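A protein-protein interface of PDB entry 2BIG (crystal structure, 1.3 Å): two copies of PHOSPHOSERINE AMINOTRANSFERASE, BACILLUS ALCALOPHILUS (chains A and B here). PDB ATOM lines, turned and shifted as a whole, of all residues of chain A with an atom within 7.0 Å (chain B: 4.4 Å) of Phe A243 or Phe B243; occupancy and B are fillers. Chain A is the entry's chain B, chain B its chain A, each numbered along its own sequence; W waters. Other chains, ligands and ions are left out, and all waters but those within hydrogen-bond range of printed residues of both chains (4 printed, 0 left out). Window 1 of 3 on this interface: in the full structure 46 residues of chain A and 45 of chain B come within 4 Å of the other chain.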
ATOM      1  N   LEU A  20      21.323  32.115   5.310  1.00  0.00           N
ATOM      2  CA  LEU A  20      22.717  32.110   4.938  1.00  0.00           C
ATOM      3  C   LEU A  20      23.576  32.765   6.016  1.00  0.00           C
ATOM      4  O   LEU A  20      24.668  32.283   6.296  1.00  0.00           O
ATOM      5  CB  LEU A  20      22.940  32.804   3.587  1.00  0.00           C
ATOM      6  CG  LEU A  20      22.661  31.905   2.378  1.00  0.00           C
ATOM      7  CD1 LEU A  20      22.560  32.692   1.103  1.00  0.00           C
ATOM      8  CD2 LEU A  20      23.736  30.824   2.225  1.00  0.00           C
ATOM      9  N   ALA A  23      23.988  30.287   8.755  1.00  0.00           N
ATOM     10  CA  ALA A  23      24.918  29.257   8.373  1.00  0.00           C
ATOM     11  C   ALA A  23      26.348  29.775   8.433  1.00  0.00           C
ATOM     12  O   ALA A  23      27.252  29.069   8.909  1.00  0.00           O
ATOM     13  CB  ALA A  23      24.619  28.765   6.965  1.00  0.00           C
ATOM     14  N   GLN A  24      26.551  31.012   7.997  1.00  0.00           N
ATOM     15  CA  GLN A  24      27.895  31.595   8.055  1.00  0.00           C
ATOM     16  C   GLN A  24      28.371  31.691   9.480  1.00  0.00           C
ATOM     17  O   GLN A  24      29.515  31.307   9.807  1.00  0.00           O
ATOM     18  CB  GLN A  24      27.897  32.978   7.398  1.00  0.00           C
ATOM     19  CG  GLN A  24      29.266  33.618   7.360  1.00  0.00           C
ATOM     20  CD  GLN A  24      29.226  35.015   6.811  1.00  0.00           C
ATOM     21  OE1 GLN A  24      28.396  35.804   7.255  1.00  0.00           O
ATOM     22  NE2 GLN A  24      30.134  35.295   5.883  1.00  0.00           N
ATOM     23  N   LEU A  27      29.347  28.237  10.925  1.00  0.00           N
ATOM     24  CA  LEU A  27      29.935  27.269  10.006  1.00  0.00           C
ATOM     25  C   LEU A  27      31.056  26.487  10.653  1.00  0.00           C
ATOM     26  O   LEU A  27      31.295  25.328  10.243  1.00  0.00           O
ATOM     27  CB  LEU A  27      30.431  27.977   8.723  1.00  0.00           C
ATOM     28  CG  LEU A  27      30.549  27.033   7.520  1.00  0.00           C
ATOM     29  CD1 LEU A  27      29.158  26.671   6.993  1.00  0.00           C
ATOM     30  CD2 LEU A  27      31.374  27.656   6.425  1.00  0.00           C
ATOM     31  N   SER A  36      31.940  21.972  12.492  1.00  0.00           N
ATOM     32  CA  SER A  36      30.941  22.365  11.535  1.00  0.00           C
ATOM     33  C   SER A  36      29.868  21.304  11.451  1.00  0.00           C
ATOM     34  O   SER A  36      30.141  20.099  11.665  1.00  0.00           O
ATOM     35  CB  SER A  36      31.607  22.440  10.142  1.00  0.00           C
ATOM     36  OG  SER A  36      30.678  22.871   9.152  1.00  0.00           O
ATOM     37  N   VAL A  37      28.671  21.694  11.051  1.00  0.00           N
ATOM     38  CA  VAL A  37      27.646  20.681  10.777  1.00  0.00           C
ATOM     39  C   VAL A  37      28.167  19.710   9.724  1.00  0.00           C
ATOM     40  O   VAL A  37      27.793  18.524   9.738  1.00  0.00           O
ATOM     41  CB  VAL A  37      26.313  21.406  10.415  1.00  0.00           C
ATOM     42  CG1 VAL A  37      26.394  22.048   9.074  1.00  0.00           C
ATOM     43  CG2 VAL A  37      25.160  20.420  10.475  1.00  0.00           C
ATOM     44  N   MET A  38      29.047  20.145   8.815  1.00  0.00           N
ATOM     45  CA  MET A  38      29.664  19.298   7.820  1.00  0.00           C
ATOM     46  C   MET A  38      30.659  18.255   8.306  1.00  0.00           C
ATOM     47  O   MET A  38      31.118  17.404   7.534  1.00  0.00           O
ATOM     48  CB  MET A  38      30.492  20.180   6.793  1.00  0.00           C
ATOM     49  CG  MET A  38      29.621  20.884   5.803  1.00  0.00           C
ATOM     50  SD  MET A  38      30.685  21.871   4.715  1.00  0.00           S
ATOM     51  CE  MET A  38      30.442  23.445   5.388  1.00  0.00           C
ATOM     52  N   TYR A  47      23.662  15.620  14.483  1.00  0.00           N
ATOM     53  CA  TYR A  47      23.080  15.689  13.144  1.00  0.00           C
ATOM     54  C   TYR A  47      21.638  15.206  13.185  1.00  0.00           C
ATOM     55  O   TYR A  47      20.776  15.740  12.497  1.00  0.00           O
ATOM     56  CB  TYR A  47      23.971  14.900  12.108  1.00  0.00           C
ATOM     57  CG  TYR A  47      23.119  14.909  10.838  1.00  0.00           C
ATOM     58  CD1 TYR A  47      23.019  16.117  10.156  1.00  0.00           C
ATOM     59  CD2 TYR A  47      22.439  13.799  10.396  1.00  0.00           C
ATOM     60  CE1 TYR A  47      22.246  16.164   8.995  1.00  0.00           C
ATOM     61  CE2 TYR A  47      21.638  13.867   9.280  1.00  0.00           C
ATOM     62  CZ  TYR A  47      21.553  15.042   8.607  1.00  0.00           C
ATOM     63  OH  TYR A  47      20.746  15.127   7.483  1.00  0.00           O
ATOM     64  N   PRO A 201      19.517  24.665  -0.913  1.00  0.00           N
ATOM     65  CA  PRO A 201      20.506  24.498  -1.953  1.00  0.00           C
ATOM     66  C   PRO A 201      20.305  23.163  -2.653  1.00  0.00           C
ATOM     67  O   PRO A 201      19.504  22.306  -2.257  1.00  0.00           O
ATOM     68  CB  PRO A 201      21.856  24.539  -1.210  1.00  0.00           C
ATOM     69  CG  PRO A 201      21.520  23.909   0.119  1.00  0.00           C
ATOM     70  CD  PRO A 201      20.125  24.416   0.414  1.00  0.00           C
ATOM     71  N   SER A 202      20.989  23.020  -3.768  1.00  0.00           N
ATOM     72  CA  SER A 202      20.917  21.782  -4.504  1.00  0.00           C
ATOM     73  C   SER A 202      21.666  20.702  -3.725  1.00  0.00           C
ATOM     74  O   SER A 202      22.561  20.956  -2.934  1.00  0.00           O
ATOM     75  CB  SER A 202      21.428  21.927  -5.941  1.00  0.00           C
ATOM     76  OG  SER A 202      22.793  22.220  -5.896  1.00  0.00           O
ATOM     77  N   VAL A 204      19.820  17.923  -2.219  1.00  0.00           N
ATOM     78  CA  VAL A 204      18.783  17.122  -1.589  1.00  0.00           C
ATOM     79  C   VAL A 204      17.458  17.314  -2.337  1.00  0.00           C
ATOM     80  O   VAL A 204      17.168  18.378  -2.867  1.00  0.00           O
ATOM     81  CB  VAL A 204      18.672  17.427  -0.094  1.00  0.00           C
ATOM     82  CG1 VAL A 204      18.144  18.831   0.174  1.00  0.00           C
ATOM     83  CG2 VAL A 204      17.833  16.350   0.637  1.00  0.00           C
ATOM     84  N   PRO A 240      23.406  10.856   4.328  1.00  0.00           N
ATOM     85  CA  PRO A 240      22.602  11.881   3.653  1.00  0.00           C
ATOM     86  C   PRO A 240      23.494  13.070   3.327  1.00  0.00           C
ATOM     87  O   PRO A 240      24.603  13.212   3.814  1.00  0.00           O
ATOM     88  CB  PRO A 240      21.539  12.224   4.678  1.00  0.00           C
ATOM     89  CG  PRO A 240      22.168  11.932   5.995  1.00  0.00           C
ATOM     90  CD  PRO A 240      23.163  10.838   5.776  1.00  0.00           C
ATOM     91  N   PRO A 241      22.926  13.976   2.504  1.00  0.00           N
ATOM     92  CA  PRO A 241      23.566  15.266   2.212  1.00  0.00           C
ATOM     93  C   PRO A 241      23.355  16.198   3.382  1.00  0.00           C
ATOM     94  O   PRO A 241      22.432  17.004   3.433  1.00  0.00           O
ATOM     95  CB  PRO A 241      22.861  15.711   0.931  1.00  0.00           C
ATOM     96  CG  PRO A 241      21.477  15.150   1.068  1.00  0.00           C
ATOM     97  CD  PRO A 241      21.680  13.781   1.724  1.00  0.00           C
ATOM     98  N   THR A 242      24.203  16.045   4.395  1.00  0.00           N
ATOM     99  CA  THR A 242      23.981  16.651   5.696  1.00  0.00           C
ATOM    100  C   THR A 242      23.903  18.177   5.660  1.00  0.00           C
ATOM    101  O   THR A 242      23.015  18.758   6.259  1.00  0.00           O
ATOM    102  CB  THR A 242      24.996  16.162   6.737  1.00  0.00           C
ATOM    103  OG1 THR A 242      26.304  16.467   6.233  1.00  0.00           O
ATOM    104  CG2 THR A 242      24.892  14.671   7.000  1.00  0.00           C
ATOM    105  N   PHE A 243      24.829  18.817   4.941  1.00  0.00           N
ATOM    106  CA  PHE A 243      24.785  20.276   4.864  1.00  0.00           C
ATOM    107  C   PHE A 243      23.566  20.760   4.112  1.00  0.00           C
ATOM    108  O   PHE A 243      22.968  21.766   4.506  1.00  0.00           O
ATOM    109  CB  PHE A 243      26.068  20.847   4.287  1.00  0.00           C
ATOM    110  CG  PHE A 243      26.125  22.357   4.430  1.00  0.00           C
ATOM    111  CD1 PHE A 243      26.402  22.924   5.667  1.00  0.00           C
ATOM    112  CD2 PHE A 243      25.867  23.166   3.361  1.00  0.00           C
ATOM    113  CE1 PHE A 243      26.441  24.302   5.791  1.00  0.00           C
ATOM    114  CE2 PHE A 243      25.934  24.538   3.473  1.00  0.00           C
ATOM    115  CZ  PHE A 243      26.190  25.099   4.712  1.00  0.00           C
ATOM    116  N   SER A 244      23.182  20.062   3.037  1.00  0.00           N
ATOM    117  CA  SER A 244      21.993  20.504   2.321  1.00  0.00           C
ATOM    118  C   SER A 244      20.740  20.411   3.191  1.00  0.00           C
ATOM    119  O   SER A 244      19.867  21.255   3.128  1.00  0.00           O
ATOM    120  CB  SER A 244      21.830  19.687   1.053  1.00  0.00           C
ATOM    121  OG  SER A 244      22.840  20.042   0.120  1.00  0.00           O
ATOM    122  N   ILE A 245      20.650  19.331   4.011  1.00  0.00           N
ATOM    123  CA  ILE A 245      19.491  19.182   4.893  1.00  0.00           C
ATOM    124  C   ILE A 245      19.520  20.221   6.014  1.00  0.00           C
ATOM    125  O   ILE A 245      18.488  20.793   6.408  1.00  0.00           O
ATOM    126  CB  ILE A 245      19.412  17.749   5.404  1.00  0.00           C
ATOM    127  CG1 ILE A 245      19.037  16.802   4.259  1.00  0.00           C
ATOM    128  CG2 ILE A 245      18.450  17.608   6.578  1.00  0.00           C
ATOM    129  CD1 ILE A 245      19.431  15.364   4.474  1.00  0.00           C
ATOM    130  N   TYR A 246      20.706  20.534   6.550  1.00  0.00           N
ATOM    131  CA  TYR A 246      20.871  21.642   7.483  1.00  0.00           C
ATOM    132  C   TYR A 246      20.373  22.943   6.879  1.00  0.00           C
ATOM    133  O   TYR A 246      19.664  23.723   7.500  1.00  0.00           O
ATOM    134  CB  TYR A 246      22.345  21.695   7.931  1.00  0.00           C
ATOM    135  CG  TYR A 246      22.718  23.026   8.533  1.00  0.00           C
ATOM    136  CD1 TYR A 246      22.509  23.291   9.867  1.00  0.00           C
ATOM    137  CD2 TYR A 246      23.300  24.030   7.770  1.00  0.00           C
ATOM    138  CE1 TYR A 246      22.851  24.495  10.421  1.00  0.00           C
ATOM    139  CE2 TYR A 246      23.622  25.260   8.312  1.00  0.00           C
ATOM    140  CZ  TYR A 246      23.410  25.492   9.645  1.00  0.00           C
ATOM    141  OH  TYR A 246      23.733  26.732  10.152  1.00  0.00           O
ATOM    142  N   MET A 247      20.783  23.253   5.663  1.00  0.00           N
ATOM    143  CA  MET A 247      20.362  24.493   5.009  1.00  0.00           C
ATOM    144  C   MET A 247      18.850  24.497   4.777  1.00  0.00           C
ATOM    145  O   MET A 247      18.205  25.519   4.921  1.00  0.00           O
ATOM    146  CB  MET A 247      21.143  24.724   3.725  1.00  0.00           C
ATOM    147  CG  MET A 247      22.550  25.150   3.813  1.00  0.00           C
ATOM    148  SD  MET A 247      22.758  26.663   4.771  1.00  0.00           S
ATOM    149  CE  MET A 247      21.592  27.752   3.974  1.00  0.00           C
ATOM    150  N   LEU A 248      18.295  23.351   4.364  1.00  0.00           N
ATOM    151  CA  LEU A 248      16.841  23.216   4.277  1.00  0.00           C
ATOM    152  C   LEU A 248      16.175  23.582   5.571  1.00  0.00           C
ATOM    153  O   LEU A 248      15.196  24.333   5.612  1.00  0.00           O
ATOM    154  CB  LEU A 248      16.537  21.785   3.850  1.00  0.00           C
ATOM    155  CG  LEU A 248      15.076  21.282   3.909  1.00  0.00           C
ATOM    156  CD1 LEU A 248      14.261  22.051   2.917  1.00  0.00           C
ATOM    157  CD2 LEU A 248      15.016  19.766   3.663  1.00  0.00           C
ATOM    158  N   ARG A 249      16.695  23.028   6.690  1.00  0.00           N
ATOM    159  CA  ARG A 249      16.156  23.371   8.000  1.00  0.00           C
ATOM    160  C   ARG A 249      16.185  24.883   8.175  1.00  0.00           C
ATOM    161  O   ARG A 249      15.182  25.507   8.626  1.00  0.00           O
ATOM    162  CB  ARG A 249      16.942  22.634   9.086  1.00  0.00           C
ATOM    163  CG  ARG A 249      16.368  22.734  10.479  1.00  0.00           C
ATOM    164  CD  ARG A 249      16.597  23.957  11.256  1.00  0.00           C
ATOM    165  NE  ARG A 249      17.969  24.463  11.312  1.00  0.00           N
ATOM    166  CZ  ARG A 249      18.862  24.272  12.276  1.00  0.00           C
ATOM    167  NH1 ARG A 249      18.657  23.540  13.379  1.00  0.00           N
ATOM    168  NH2 ARG A 249      20.046  24.842  12.081  1.00  0.00           N
ATOM    169  N   LEU B  27      30.846  32.983   2.080  1.00  0.00           N
ATOM    170  CA  LEU B  27      29.550  32.291   2.014  1.00  0.00           C
ATOM    171  C   LEU B  27      28.439  33.164   1.434  1.00  0.00           C
ATOM    172  O   LEU B  27      27.524  32.608   0.839  1.00  0.00           O
ATOM    173  CB  LEU B  27      29.078  31.752   3.367  1.00  0.00           C
ATOM    174  CG  LEU B  27      28.107  30.608   3.279  1.00  0.00           C
ATOM    175  CD1 LEU B  27      28.786  29.312   2.850  1.00  0.00           C
ATOM    176  CD2 LEU B  27      27.449  30.354   4.610  1.00  0.00           C
ATOM    177  N   VAL B  37      27.893  30.776  -3.389  1.00  0.00           N
ATOM    178  CA  VAL B  37      28.076  29.747  -4.378  1.00  0.00           C
ATOM    179  C   VAL B  37      26.806  28.909  -4.422  1.00  0.00           C
ATOM    180  O   VAL B  37      26.493  28.409  -5.508  1.00  0.00           O
ATOM    181  CB  VAL B  37      29.420  28.960  -4.116  1.00  0.00           C
ATOM    182  CG1 VAL B  37      29.227  28.140  -2.901  1.00  0.00           C
ATOM    183  CG2 VAL B  37      29.793  28.132  -5.323  1.00  0.00           C
ATOM    184  N   MET B  38      26.045  28.752  -3.349  1.00  0.00           N
ATOM    185  CA  MET B  38      24.799  28.016  -3.212  1.00  0.00           C
ATOM    186  C   MET B  38      23.637  28.643  -3.951  1.00  0.00           C
ATOM    187  O   MET B  38      22.591  27.999  -4.117  1.00  0.00           O
ATOM    188  CB  MET B  38      24.319  27.887  -1.709  1.00  0.00           C
ATOM    189  CG  MET B  38      24.982  26.768  -0.957  1.00  0.00           C
ATOM    190  SD  MET B  38      24.219  27.024   0.659  1.00  0.00           S
ATOM    191  CE  MET B  38      25.616  27.734   1.448  1.00  0.00           C
ATOM    192  N   PRO B 241      25.387  18.930  -7.055  1.00  0.00           N
ATOM    193  CA  PRO B 241      25.471  19.369  -5.637  1.00  0.00           C
ATOM    194  C   PRO B 241      26.568  20.431  -5.553  1.00  0.00           C
ATOM    195  O   PRO B 241      27.723  20.159  -5.255  1.00  0.00           O
ATOM    196  CB  PRO B 241      25.789  18.078  -4.918  1.00  0.00           C
ATOM    197  CG  PRO B 241      26.606  17.277  -5.883  1.00  0.00           C
ATOM    198  CD  PRO B 241      25.964  17.596  -7.225  1.00  0.00           C
ATOM    199  N   THR B 242      26.174  21.668  -5.873  1.00  0.00           N
ATOM    200  CA  THR B 242      27.167  22.686  -6.135  1.00  0.00           C
ATOM    201  C   THR B 242      27.989  23.043  -4.908  1.00  0.00           C
ATOM    202  O   THR B 242      29.213  23.221  -5.015  1.00  0.00           O
ATOM    203  CB  THR B 242      26.519  23.957  -6.707  1.00  0.00           C
ATOM    204  OG1 THR B 242      25.475  24.369  -5.830  1.00  0.00           O
ATOM    205  CG2 THR B 242      25.943  23.788  -8.109  1.00  0.00           C
ATOM    206  N   PHE B 243      27.341  23.156  -3.737  1.00  0.00           N
ATOM    207  CA  PHE B 243      28.116  23.485  -2.549  1.00  0.00           C
ATOM    208  C   PHE B 243      29.063  22.331  -2.184  1.00  0.00           C
ATOM    209  O   PHE B 243      30.194  22.603  -1.754  1.00  0.00           O
ATOM    210  CB  PHE B 243      27.235  23.851  -1.376  1.00  0.00           C
ATOM    211  CG  PHE B 243      28.048  24.475  -0.228  1.00  0.00           C
ATOM    212  CD1 PHE B 243      28.559  25.754  -0.345  1.00  0.00           C
ATOM    213  CD2 PHE B 243      28.269  23.789   0.941  1.00  0.00           C
ATOM    214  CE1 PHE B 243      29.294  26.320   0.684  1.00  0.00           C
ATOM    215  CE2 PHE B 243      29.001  24.335   1.965  1.00  0.00           C
ATOM    216  CZ  PHE B 243      29.483  25.606   1.837  1.00  0.00           C
ATOM    217  N   SER B 244      28.613  21.094  -2.324  1.00  0.00           N
ATOM    218  CA  SER B 244      29.529  20.000  -1.985  1.00  0.00           C
ATOM    219  C   SER B 244      30.730  20.002  -2.928  1.00  0.00           C
ATOM    220  O   SER B 244      31.830  19.724  -2.465  1.00  0.00           O
ATOM    221  CB  SER B 244      28.812  18.644  -2.061  1.00  0.00           C
ATOM    222  OG  SER B 244      27.802  18.572  -1.090  1.00  0.00           O
ATOM    223  N   ILE B 245      30.501  20.262  -4.232  1.00  0.00           N
ATOM    224  CA  ILE B 245      31.643  20.273  -5.168  1.00  0.00           C
ATOM    225  C   ILE B 245      32.559  21.452  -4.884  1.00  0.00           C
ATOM    226  O   ILE B 245      33.795  21.316  -4.974  1.00  0.00           O
ATOM    227  CB  ILE B 245      31.119  20.235  -6.611  1.00  0.00           C
ATOM    228  CG1 ILE B 245      30.446  18.883  -6.873  1.00  0.00           C
ATOM    229  CG2 ILE B 245      32.203  20.558  -7.612  1.00  0.00           C
ATOM    230  CD1 ILE B 245      29.539  18.877  -8.095  1.00  0.00           C
ATOM    231  N   TYR B 246      32.026  22.606  -4.525  1.00  0.00           N
ATOM    232  CA  TYR B 246      32.800  23.743  -4.053  1.00  0.00           C
ATOM    233  C   TYR B 246      33.648  23.352  -2.852  1.00  0.00           C
ATOM    234  O   TYR B 246      34.847  23.668  -2.791  1.00  0.00           O
ATOM    235  CB  TYR B 246      31.831  24.909  -3.746  1.00  0.00           C
ATOM    236  CG  TYR B 246      32.453  25.977  -2.897  1.00  0.00           C
ATOM    237  CD1 TYR B 246      33.243  26.983  -3.447  1.00  0.00           C
ATOM    238  CD2 TYR B 246      32.254  25.999  -1.523  1.00  0.00           C
ATOM    239  CE1 TYR B 246      33.792  27.963  -2.651  1.00  0.00           C
ATOM    240  CE2 TYR B 246      32.841  26.962  -0.752  1.00  0.00           C
ATOM    241  CZ  TYR B 246      33.604  27.942  -1.314  1.00  0.00           C
ATOM    242  OH  TYR B 246      34.180  28.878  -0.462  1.00  0.00           O
ATOM    243  N   MET B 247      33.062  22.710  -1.848  1.00  0.00           N
ATOM    244  CA  MET B 247      33.837  22.325  -0.676  1.00  0.00           C
ATOM    245  C   MET B 247      34.914  21.335  -1.036  1.00  0.00           C
ATOM    246  O   MET B 247      36.041  21.402  -0.499  1.00  0.00           O
ATOM    247  CB  MET B 247      32.918  21.798   0.409  1.00  0.00           C
ATOM    248  CG  MET B 247      32.089  22.808   1.153  1.00  0.00           C
ATOM    249  SD  MET B 247      33.039  24.101   1.955  1.00  0.00           S
ATOM    250  CE  MET B 247      34.149  23.176   2.937  1.00  0.00           C
HETATM  251  O   HOH W   1      22.778  25.197  -4.504  1.00  0.00           O
HETATM  252  O   HOH W   2      24.680  18.178  -1.113  1.00  0.00           O
HETATM  253  O   HOH W   3      24.350  23.104  -3.119  1.00  0.00           O
HETATM  254  O   HOH W   4      25.715  20.449  -2.517  1.00  0.00           O
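The backbone NH (N) of Thr B242 sits at hydrogen-bond distance from the side-chain hydroxyl (OG) of Ser A202, 3.4 Å away.
N of Met A38 lies close to OG of Ser A36 (3.2 Å).
OG of Ser A244 sits at hydrogen-bond distance from O of Ser A202.
O of Leu A20 touches CD2 of Leu B27, at 3.8 Å.
CE of Met B38 touches CD2 of Leu A20, at 3.7 Å.
N of Gln A24 touches CD2 of Leu B27 (3.6 Å).
CE of Met A38 touches CE2 of Phe B243, at 3.8 Å.
CG of Met B247 touches SD of Met A38, at 3.9 Å.
Pro A201 touches Met B38.
Ser A202 touches Pro B241.
Met B38 touches Phe A243.
Phe A243 touches Phe B243.
Phe A243 touches two residues of chain B.
Of the printed residues of chain B, Pro A201 touches Met B38 (3.8 Å).
Printed residues of chain A within 4 Å of Met B38: Leu A20 (3.7 Å), Pro A201 (3.8 Å) and Phe A243 (3.8 Å).
Of the printed residues of chain A, Met B247 touches Met A38.
Leu A248 touches none of the printed residues of chain B.
The nearest printed residue of chain B that does not touch Phe A243 is Leu B27 (5.3 Å).
Of the 10 printed residues of chain B, 6 touch a printed residue of chain A.
Hydrophobic or aromatic side chains of chain A within 4 Å of the printed part of chain B: Leu A20, Met A38, Pro A201 and Phe A243.
Among the printed residues, 10 pairs touch across the chains.
Among the printed residues, no Asp or Glu carboxylate lies within 4 Å of a Lys or Arg side-chain nitrogen of the other chain.
Met A38 touches Phe B243, and with the chains exchanged Phe A243 touches Met B38.
Met A38 touches Met B247, but with the chains exchanged Met A247 does not touch Met B38 (4.03 Å).
Phe A243 touches its own counterpart, Phe B243.
10 positions are printed for both chains.
Of the 10 pairs that touch across the chains among the printed residues, 3 have their exchanged pair printed and touching as well.
Water W3 lies within hydrogen-bond range of O of Ser A202 (2.8 Å), N of Phe B243 (3.1 Å) and OG1 of Thr B242 (3.2 Å).
Water W1 lies within hydrogen-bond range of O of Met B38, N of Ser A202 and OG1 of Thr B242.
Water W2 bridges the side-chain hydroxyl of Ser A244 (2.9 Å) and the side-chain hydroxyl of Ser B244 (3.1 Å).
Water W4 lies within hydrogen-bond range of N of Ser B244 (3.0 Å), O of Ser A202 (3.2 Å), N of Phe B243 (3.4 Å) and O of Pro B241 (3.4 Å).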
